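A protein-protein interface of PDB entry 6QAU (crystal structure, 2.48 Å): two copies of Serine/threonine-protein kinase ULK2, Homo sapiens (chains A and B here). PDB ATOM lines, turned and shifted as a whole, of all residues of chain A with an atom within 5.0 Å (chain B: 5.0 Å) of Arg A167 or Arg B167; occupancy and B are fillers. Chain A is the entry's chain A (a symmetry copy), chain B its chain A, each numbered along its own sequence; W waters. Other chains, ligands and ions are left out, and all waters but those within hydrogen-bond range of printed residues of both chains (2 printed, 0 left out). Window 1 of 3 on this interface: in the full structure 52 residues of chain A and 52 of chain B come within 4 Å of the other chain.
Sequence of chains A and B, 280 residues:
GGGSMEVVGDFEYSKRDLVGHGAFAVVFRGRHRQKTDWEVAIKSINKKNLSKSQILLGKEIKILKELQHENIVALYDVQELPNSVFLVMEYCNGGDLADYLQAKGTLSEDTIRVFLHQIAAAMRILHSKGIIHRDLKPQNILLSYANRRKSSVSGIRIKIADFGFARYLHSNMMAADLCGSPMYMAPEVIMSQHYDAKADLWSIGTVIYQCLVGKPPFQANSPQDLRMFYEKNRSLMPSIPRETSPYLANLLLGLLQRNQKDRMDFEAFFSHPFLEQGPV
N of Arg A167 sits at hydrogen-bond distance from O of Ile A132. NH2 of Arg A167 lies within hydrogen-bond range of ND1 of His A194 (3.1 Å). NH2 of Arg B167 lies within salt-bridge range of OD1 of Asp B196. The guanidinium group of Arg A167 is in salt-bridge range of the side-chain carboxylate of Asp A196 (2.8 Å). A ring nitrogen (ND1) of His B194 lies within hydrogen-bond range of the guanidinium group (NH2) of Arg B167, 3.1 Å away. The backbone carbonyl oxygen (O) of Ile B132 sits at hydrogen-bond distance from the backbone NH (N) of Arg B167 (3.0 Å).
Arg B167 touches Arg A167 (NH1 to NE, 3.7 Å).
Arg A167 touches one residue of chain B. Arg B167 touches just one residue of chain A: Arg A167. The nearest printed residue of chain B that does not touch Arg A167 is Asp B196 (5.2 Å).
Printed residues of chain B that touch a printed residue of chain A: Arg B167. Among the printed residues, 1 pair touches across the chains. Among the printed residues, no Asp or Glu carboxylate lies within 4 Å of a Lys or Arg side-chain nitrogen of the other chain.
Arg B167 touches its own counterpart, Arg A167.
Water W1 lies within hydrogen-bond range of a ring nitrogen (ND1) of His A194 (3.2 Å), the guanidinium group of Arg A167 (3.3 Å) and the side-chain carboxylate of Asp B196 (3.5 Å). Water W2 lies within hydrogen-bond range of a ring nitrogen (ND1) of His B194, the guanidinium group (NH2) of Arg B167 and the side-chain carboxylate (OD1) of Asp A196.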
ATOM      1  N   ILE A  63      31.879  10.695  30.407  1.00  0.00           N
ATOM      2  CA  ILE A  63      32.600  11.940  30.311  1.00  0.00           C
ATOM      3  C   ILE A  63      33.986  11.762  30.955  1.00  0.00           C
ATOM      4  O   ILE A  63      34.998  12.063  30.326  1.00  0.00           O
ATOM      5  CB  ILE A  63      31.792  13.116  30.898  1.00  0.00           C
ATOM      6  CG1 ILE A  63      30.674  13.511  29.939  1.00  0.00           C
ATOM      7  CG2 ILE A  63      32.698  14.301  31.217  1.00  0.00           C
ATOM      8  CD1 ILE A  63      29.678  14.487  30.487  1.00  0.00           C
ATOM      9  N   GLY A 130      33.790  18.928  23.017  1.00  0.00           N
ATOM     10  CA  GLY A 130      32.507  19.596  23.063  1.00  0.00           C
ATOM     11  C   GLY A 130      31.742  19.313  24.346  1.00  0.00           C
ATOM     12  O   GLY A 130      30.547  19.053  24.295  1.00  0.00           O
ATOM     13  N   ILE A 131      32.413  19.363  25.497  1.00  0.00           N
ATOM     14  CA  ILE A 131      31.764  19.207  26.776  1.00  0.00           C
ATOM     15  C   ILE A 131      31.787  20.537  27.528  1.00  0.00           C
ATOM     16  O   ILE A 131      32.809  21.233  27.533  1.00  0.00           O
ATOM     17  CB  ILE A 131      32.441  18.105  27.589  1.00  0.00           C
ATOM     18  CG1 ILE A 131      32.333  16.742  26.900  1.00  0.00           C
ATOM     19  CG2 ILE A 131      31.901  18.081  29.010  1.00  0.00           C
ATOM     20  CD1 ILE A 131      33.248  15.688  27.483  1.00  0.00           C
ATOM     21  N   ILE A 132      30.651  20.877  28.159  1.00  0.00           N
ATOM     22  CA  ILE A 132      30.595  21.983  29.100  1.00  0.00           C
ATOM     23  C   ILE A 132      30.183  21.430  30.449  1.00  0.00           C
ATOM     24  O   ILE A 132      29.416  20.505  30.518  1.00  0.00           O
ATOM     25  CB  ILE A 132      29.664  23.107  28.638  1.00  0.00           C
ATOM     26  CG1 ILE A 132      28.199  22.657  28.534  1.00  0.00           C
ATOM     27  CG2 ILE A 132      30.165  23.667  27.336  1.00  0.00           C
ATOM     28  CD1 ILE A 132      27.269  23.681  27.832  1.00  0.00           C
ATOM     29  N   ARG A 134      29.144  23.318  33.401  1.00  0.00           N
ATOM     30  CA  ARG A 134      27.923  24.102  33.731  1.00  0.00           C
ATOM     31  C   ARG A 134      27.756  24.364  35.226  1.00  0.00           C
ATOM     32  O   ARG A 134      26.930  25.141  35.592  1.00  0.00           O
ATOM     33  CB  ARG A 134      26.666  23.439  33.195  1.00  0.00           C
ATOM     34  CG  ARG A 134      26.578  23.463  31.684  1.00  0.00           C
ATOM     35  CD  ARG A 134      25.667  22.417  31.138  1.00  0.00           C
ATOM     36  NE  ARG A 134      24.340  22.896  31.001  1.00  0.00           N
ATOM     37  CZ  ARG A 134      23.299  22.285  31.490  1.00  0.00           C
ATOM     38  NH1 ARG A 134      23.401  21.025  31.871  1.00  0.00           N
ATOM     39  NH2 ARG A 134      22.174  22.964  31.658  1.00  0.00           N
ATOM     40  N   PHE A 165      26.371  17.668  36.047  1.00  0.00           N
ATOM     41  CA  PHE A 165      25.462  18.623  35.394  1.00  0.00           C
ATOM     42  C   PHE A 165      25.994  19.014  34.004  1.00  0.00           C
ATOM     43  O   PHE A 165      25.488  19.925  33.361  1.00  0.00           O
ATOM     44  CB  PHE A 165      25.214  19.821  36.313  1.00  0.00           C
ATOM     45  CG  PHE A 165      24.033  20.695  35.925  1.00  0.00           C
ATOM     46  CD1 PHE A 165      22.758  20.148  35.794  1.00  0.00           C
ATOM     47  CD2 PHE A 165      24.175  22.070  35.715  1.00  0.00           C
ATOM     48  CE1 PHE A 165      21.675  20.939  35.431  1.00  0.00           C
ATOM     49  CE2 PHE A 165      23.094  22.852  35.336  1.00  0.00           C
ATOM     50  CZ  PHE A 165      21.846  22.284  35.187  1.00  0.00           C
ATOM     51  N   ALA A 166      26.984  18.264  33.516  1.00  0.00           N
ATOM     52  CA  ALA A 166      27.664  18.574  32.266  1.00  0.00           C
ATOM     53  C   ALA A 166      26.798  18.158  31.069  1.00  0.00           C
ATOM     54  O   ALA A 166      25.907  17.342  31.192  1.00  0.00           O
ATOM     55  CB  ALA A 166      29.006  17.902  32.241  1.00  0.00           C
ATOM     56  N   ARG A 167      27.103  18.708  29.894  1.00  0.00           N
ATOM     57  CA  ARG A 167      26.416  18.268  28.698  1.00  0.00           C
ATOM     58  C   ARG A 167      27.372  18.301  27.497  1.00  0.00           C
ATOM     59  O   ARG A 167      28.389  18.983  27.514  1.00  0.00           O
ATOM     60  CB  ARG A 167      25.112  19.061  28.525  1.00  0.00           C
ATOM     61  CG  ARG A 167      25.176  20.316  27.673  1.00  0.00           C
ATOM     62  CD  ARG A 167      23.781  20.804  27.302  1.00  0.00           C
ATOM     63  NE  ARG A 167      23.779  22.020  26.482  1.00  0.00           N
ATOM     64  CZ  ARG A 167      23.557  22.046  25.168  1.00  0.00           C
ATOM     65  NH1 ARG A 167      23.313  20.918  24.512  1.00  0.00           N
ATOM     66  NH2 ARG A 167      23.603  23.190  24.505  1.00  0.00           N
ATOM     67  N   TYR A 168      27.041  17.460  26.510  1.00  0.00           N
ATOM     68  CA  TYR A 168      27.700  17.422  25.219  1.00  0.00           C
ATOM     69  C   TYR A 168      27.053  18.437  24.266  1.00  0.00           C
ATOM     70  O   TYR A 168      25.868  18.581  24.240  1.00  0.00           O
ATOM     71  CB  TYR A 168      27.605  16.020  24.622  1.00  0.00           C
ATOM     72  CG  TYR A 168      28.518  14.989  25.235  1.00  0.00           C
ATOM     73  CD1 TYR A 168      29.844  14.906  24.862  1.00  0.00           C
ATOM     74  CD2 TYR A 168      28.041  14.047  26.136  1.00  0.00           C
ATOM     75  CE1 TYR A 168      30.684  13.950  25.395  1.00  0.00           C
ATOM     76  CE2 TYR A 168      28.873  13.084  26.688  1.00  0.00           C
ATOM     77  CZ  TYR A 168      30.201  13.032  26.305  1.00  0.00           C
ATOM     78  OH  TYR A 168      31.052  12.065  26.782  1.00  0.00           O
ATOM     79  N   LEU A 169      27.891  19.183  23.544  1.00  0.00           N
ATOM     80  CA  LEU A 169      27.502  19.970  22.344  1.00  0.00           C
ATOM     81  C   LEU A 169      27.905  19.216  21.062  1.00  0.00           C
ATOM     82  O   LEU A 169      29.124  18.956  20.820  1.00  0.00           O
ATOM     83  CB  LEU A 169      28.242  21.311  22.371  1.00  0.00           C
ATOM     84  CG  LEU A 169      28.204  22.073  23.681  1.00  0.00           C
ATOM     85  CD1 LEU A 169      29.077  23.299  23.562  1.00  0.00           C
ATOM     86  CD2 LEU A 169      26.784  22.445  24.073  1.00  0.00           C
ATOM     87  N   HIS A 194      24.466  27.244  20.259  1.00  0.00           N
ATOM     88  CA  HIS A 194      24.347  26.834  21.650  1.00  0.00           C
ATOM     89  C   HIS A 194      24.483  28.050  22.559  1.00  0.00           C
ATOM     90  O   HIS A 194      25.522  28.691  22.606  1.00  0.00           O
ATOM     91  CB  HIS A 194      25.426  25.806  21.979  1.00  0.00           C
ATOM     92  CG  HIS A 194      25.264  24.519  21.251  1.00  0.00           C
ATOM     93  ND1 HIS A 194      24.187  23.679  21.480  1.00  0.00           N
ATOM     94  CD2 HIS A 194      26.027  23.917  20.318  1.00  0.00           C
ATOM     95  CE1 HIS A 194      24.309  22.607  20.727  1.00  0.00           C
ATOM     96  NE2 HIS A 194      25.438  22.722  20.013  1.00  0.00           N
ATOM     97  N   ASP A 196      24.701  28.159  25.720  1.00  0.00           N
ATOM     98  CA  ASP A 196      25.424  27.886  26.963  1.00  0.00           C
ATOM     99  C   ASP A 196      26.859  27.435  26.671  1.00  0.00           C
ATOM    100  O   ASP A 196      27.524  26.990  27.550  1.00  0.00           O
ATOM    101  CB  ASP A 196      24.700  26.839  27.814  1.00  0.00           C
ATOM    102  CG  ASP A 196      24.407  25.514  27.117  1.00  0.00           C
ATOM    103  OD1 ASP A 196      24.643  25.415  25.889  1.00  0.00           O
ATOM    104  OD2 ASP A 196      23.966  24.582  27.817  1.00  0.00           O
ATOM    105  N   ILE B  63      13.511   8.470  28.325  1.00  0.00           N
ATOM    106  CA  ILE B  63      12.611   9.397  27.688  1.00  0.00           C
ATOM    107  C   ILE B  63      11.300   8.665  27.350  1.00  0.00           C
ATOM    108  O   ILE B  63      10.225   9.131  27.721  1.00  0.00           O
ATOM    109  CB  ILE B  63      13.264  10.084  26.470  1.00  0.00           C
ATOM    110  CG1 ILE B  63      14.262  11.138  26.940  1.00  0.00           C
ATOM    111  CG2 ILE B  63      12.210  10.688  25.547  1.00  0.00           C
ATOM    112  CD1 ILE B  63      15.130  11.720  25.866  1.00  0.00           C
ATOM    113  N   GLY B 130      10.038  19.098  29.340  1.00  0.00           N
ATOM    114  CA  GLY B 130      11.209  19.783  28.837  1.00  0.00           C
ATOM    115  C   GLY B 130      12.072  18.901  27.948  1.00  0.00           C
ATOM    116  O   GLY B 130      13.287  18.905  28.086  1.00  0.00           O
ATOM    117  N   ILE B 131      11.458  18.147  27.035  1.00  0.00           N
ATOM    118  CA  ILE B 131      12.186  17.350  26.079  1.00  0.00           C
ATOM    119  C   ILE B 131      12.004  17.935  24.679  1.00  0.00           C
ATOM    120  O   ILE B 131      10.893  18.327  24.306  1.00  0.00           O
ATOM    121  CB  ILE B 131      11.721  15.895  26.129  1.00  0.00           C
ATOM    122  CG1 ILE B 131      11.994  15.258  27.493  1.00  0.00           C
ATOM    123  CG2 ILE B 131      12.329  15.100  24.985  1.00  0.00           C
ATOM    124  CD1 ILE B 131      11.275  13.944  27.711  1.00  0.00           C
ATOM    125  N   ILE B 132      13.107  17.990  23.914  1.00  0.00           N
ATOM    126  CA  ILE B 132      13.046  18.297  22.496  1.00  0.00           C
ATOM    127  C   ILE B 132      13.603  17.112  21.735  1.00  0.00           C
ATOM    128  O   ILE B 132      14.500  16.458  22.200  1.00  0.00           O
ATOM    129  CB  ILE B 132      13.777  19.596  22.139  1.00  0.00           C
ATOM    130  CG1 ILE B 132      15.285  19.521  22.421  1.00  0.00           C
ATOM    131  CG2 ILE B 132      13.135  20.745  22.864  1.00  0.00           C
ATOM    132  CD1 ILE B 132      16.018  20.885  22.315  1.00  0.00           C
ATOM    133  N   ARG B 134      14.498  16.966  18.194  1.00  0.00           N
ATOM    134  CA  ARG B 134      15.604  17.562  17.397  1.00  0.00           C
ATOM    135  C   ARG B 134      15.805  16.890  16.040  1.00  0.00           C
ATOM    136  O   ARG B 134      16.525  17.401  15.240  1.00  0.00           O
ATOM    137  CB  ARG B 134      16.917  17.551  18.161  1.00  0.00           C
ATOM    138  CG  ARG B 134      16.925  18.493  19.345  1.00  0.00           C
ATOM    139  CD  ARG B 134      17.951  18.137  20.365  1.00  0.00           C
ATOM    140  NE  ARG B 134      19.185  18.792  20.119  1.00  0.00           N
ATOM    141  CZ  ARG B 134      20.328  18.172  20.046  1.00  0.00           C
ATOM    142  NH1 ARG B 134      20.433  16.939  20.508  1.00  0.00           N
ATOM    143  NH2 ARG B 134      21.348  18.769  19.447  1.00  0.00           N
ATOM    144  N   PHE B 165      18.204  11.350  19.356  1.00  0.00           N
ATOM    145  CA  PHE B 165      18.928  12.627  19.254  1.00  0.00           C
ATOM    146  C   PHE B 165      18.275  13.694  20.151  1.00  0.00           C
ATOM    147  O   PHE B 165      18.608  14.869  20.089  1.00  0.00           O
ATOM    148  CB  PHE B 165      19.041  13.048  17.787  1.00  0.00           C
ATOM    149  CG  PHE B 165      20.060  14.143  17.511  1.00  0.00           C
ATOM    150  CD1 PHE B 165      21.393  13.981  17.881  1.00  0.00           C
ATOM    151  CD2 PHE B 165      19.706  15.326  16.855  1.00  0.00           C
ATOM    152  CE1 PHE B 165      22.328  14.980  17.639  1.00  0.00           C
ATOM    153  CE2 PHE B 165      20.639  16.328  16.632  1.00  0.00           C
ATOM    154  CZ  PHE B 165      21.948  16.156  17.031  1.00  0.00           C
ATOM    155  N   ALA B 166      17.384  13.253  21.041  1.00  0.00           N
ATOM    156  CA  ALA B 166      16.604  14.150  21.884  1.00  0.00           C
ATOM    157  C   ALA B 166      17.461  14.673  23.045  1.00  0.00           C
ATOM    158  O   ALA B 166      18.467  14.090  23.394  1.00  0.00           O
ATOM    159  CB  ALA B 166      15.376  13.439  22.376  1.00  0.00           C
ATOM    160  N   ARG B 167      17.020  15.767  23.664  1.00  0.00           N
ATOM    161  CA  ARG B 167      17.703  16.245  24.847  1.00  0.00           C
ATOM    162  C   ARG B 167      16.695  16.854  25.831  1.00  0.00           C
ATOM    163  O   ARG B 167      15.590  17.228  25.457  1.00  0.00           O
ATOM    164  CB  ARG B 167      18.865  17.163  24.442  1.00  0.00           C
ATOM    165  CG  ARG B 167      18.574  18.652  24.367  1.00  0.00           C
ATOM    166  CD  ARG B 167      19.862  19.465  24.298  1.00  0.00           C
ATOM    167  NE  ARG B 167      19.643  20.912  24.218  1.00  0.00           N
ATOM    168  CZ  ARG B 167      19.793  21.758  25.237  1.00  0.00           C
ATOM    169  NH1 ARG B 167      20.168  21.305  26.428  1.00  0.00           N
ATOM    170  NH2 ARG B 167      19.545  23.047  25.078  1.00  0.00           N
ATOM    171  N   TYR B 168      17.096  16.839  27.108  1.00  0.00           N
ATOM    172  CA  TYR B 168      16.387  17.490  28.191  1.00  0.00           C
ATOM    173  C   TYR B 168      16.828  18.956  28.306  1.00  0.00           C
ATOM    174  O   TYR B 168      17.975  19.258  28.181  1.00  0.00           O
ATOM    175  CB  TYR B 168      16.658  16.764  29.507  1.00  0.00           C
ATOM    176  CG  TYR B 168      15.939  15.451  29.687  1.00  0.00           C
ATOM    177  CD1 TYR B 168      14.623  15.415  30.100  1.00  0.00           C
ATOM    178  CD2 TYR B 168      16.594  14.241  29.513  1.00  0.00           C
ATOM    179  CE1 TYR B 168      13.960  14.221  30.294  1.00  0.00           C
ATOM    180  CE2 TYR B 168      15.942  13.029  29.696  1.00  0.00           C
ATOM    181  CZ  TYR B 168      14.620  13.023  30.098  1.00  0.00           C
ATOM    182  OH  TYR B 168      13.945  11.852  30.344  1.00  0.00           O
ATOM    183  N   LEU B 169      15.854  19.852  28.473  1.00  0.00           N
ATOM    184  CA  LEU B 169      16.062  21.250  28.935  1.00  0.00           C
ATOM    185  C   LEU B 169      15.711  21.372  30.430  1.00  0.00           C
ATOM    186  O   LEU B 169      14.534  21.133  30.840  1.00  0.00           O
ATOM    187  CB  LEU B 169      15.135  22.175  28.142  1.00  0.00           C
ATOM    188  CG  LEU B 169      15.124  21.988  26.637  1.00  0.00           C
ATOM    189  CD1 LEU B 169      14.075  22.893  26.036  1.00  0.00           C
ATOM    190  CD2 LEU B 169      16.492  22.254  26.030  1.00  0.00           C
ATOM    191  N   HIS B 194      17.882  28.658  26.057  1.00  0.00           N
ATOM    192  CA  HIS B 194      18.130  27.516  25.191  1.00  0.00           C
ATOM    193  C   HIS B 194      17.860  27.902  23.740  1.00  0.00           C
ATOM    194  O   HIS B 194      16.742  28.222  23.369  1.00  0.00           O
ATOM    195  CB  HIS B 194      17.231  26.353  25.602  1.00  0.00           C
ATOM    196  CG  HIS B 194      17.546  25.807  26.950  1.00  0.00           C
ATOM    197  ND1 HIS B 194      18.745  25.169  27.221  1.00  0.00           N
ATOM    198  CD2 HIS B 194      16.834  25.783  28.095  1.00  0.00           C
ATOM    199  CE1 HIS B 194      18.745  24.764  28.473  1.00  0.00           C
ATOM    200  NE2 HIS B 194      17.577  25.117  29.029  1.00  0.00           N
ATOM    201  N   ASP B 196      17.787  26.049  21.169  1.00  0.00           N
ATOM    202  CA  ASP B 196      17.175  24.978  20.381  1.00  0.00           C
ATOM    203  C   ASP B 196      15.809  24.588  20.956  1.00  0.00           C
ATOM    204  O   ASP B 196      15.263  23.612  20.558  1.00  0.00           O
ATOM    205  CB  ASP B 196      18.087  23.751  20.297  1.00  0.00           C
ATOM    206  CG  ASP B 196      18.538  23.176  21.637  1.00  0.00           C
ATOM    207  OD1 ASP B 196      18.259  23.804  22.686  1.00  0.00           O
ATOM    208  OD2 ASP B 196      19.147  22.089  21.619  1.00  0.00           O
HETATM  209  O   HOH W   1      21.550  24.986  22.629  1.00  0.00           O
HETATM  210  O   HOH W   2      21.214  25.890  25.386  1.00  0.00           O
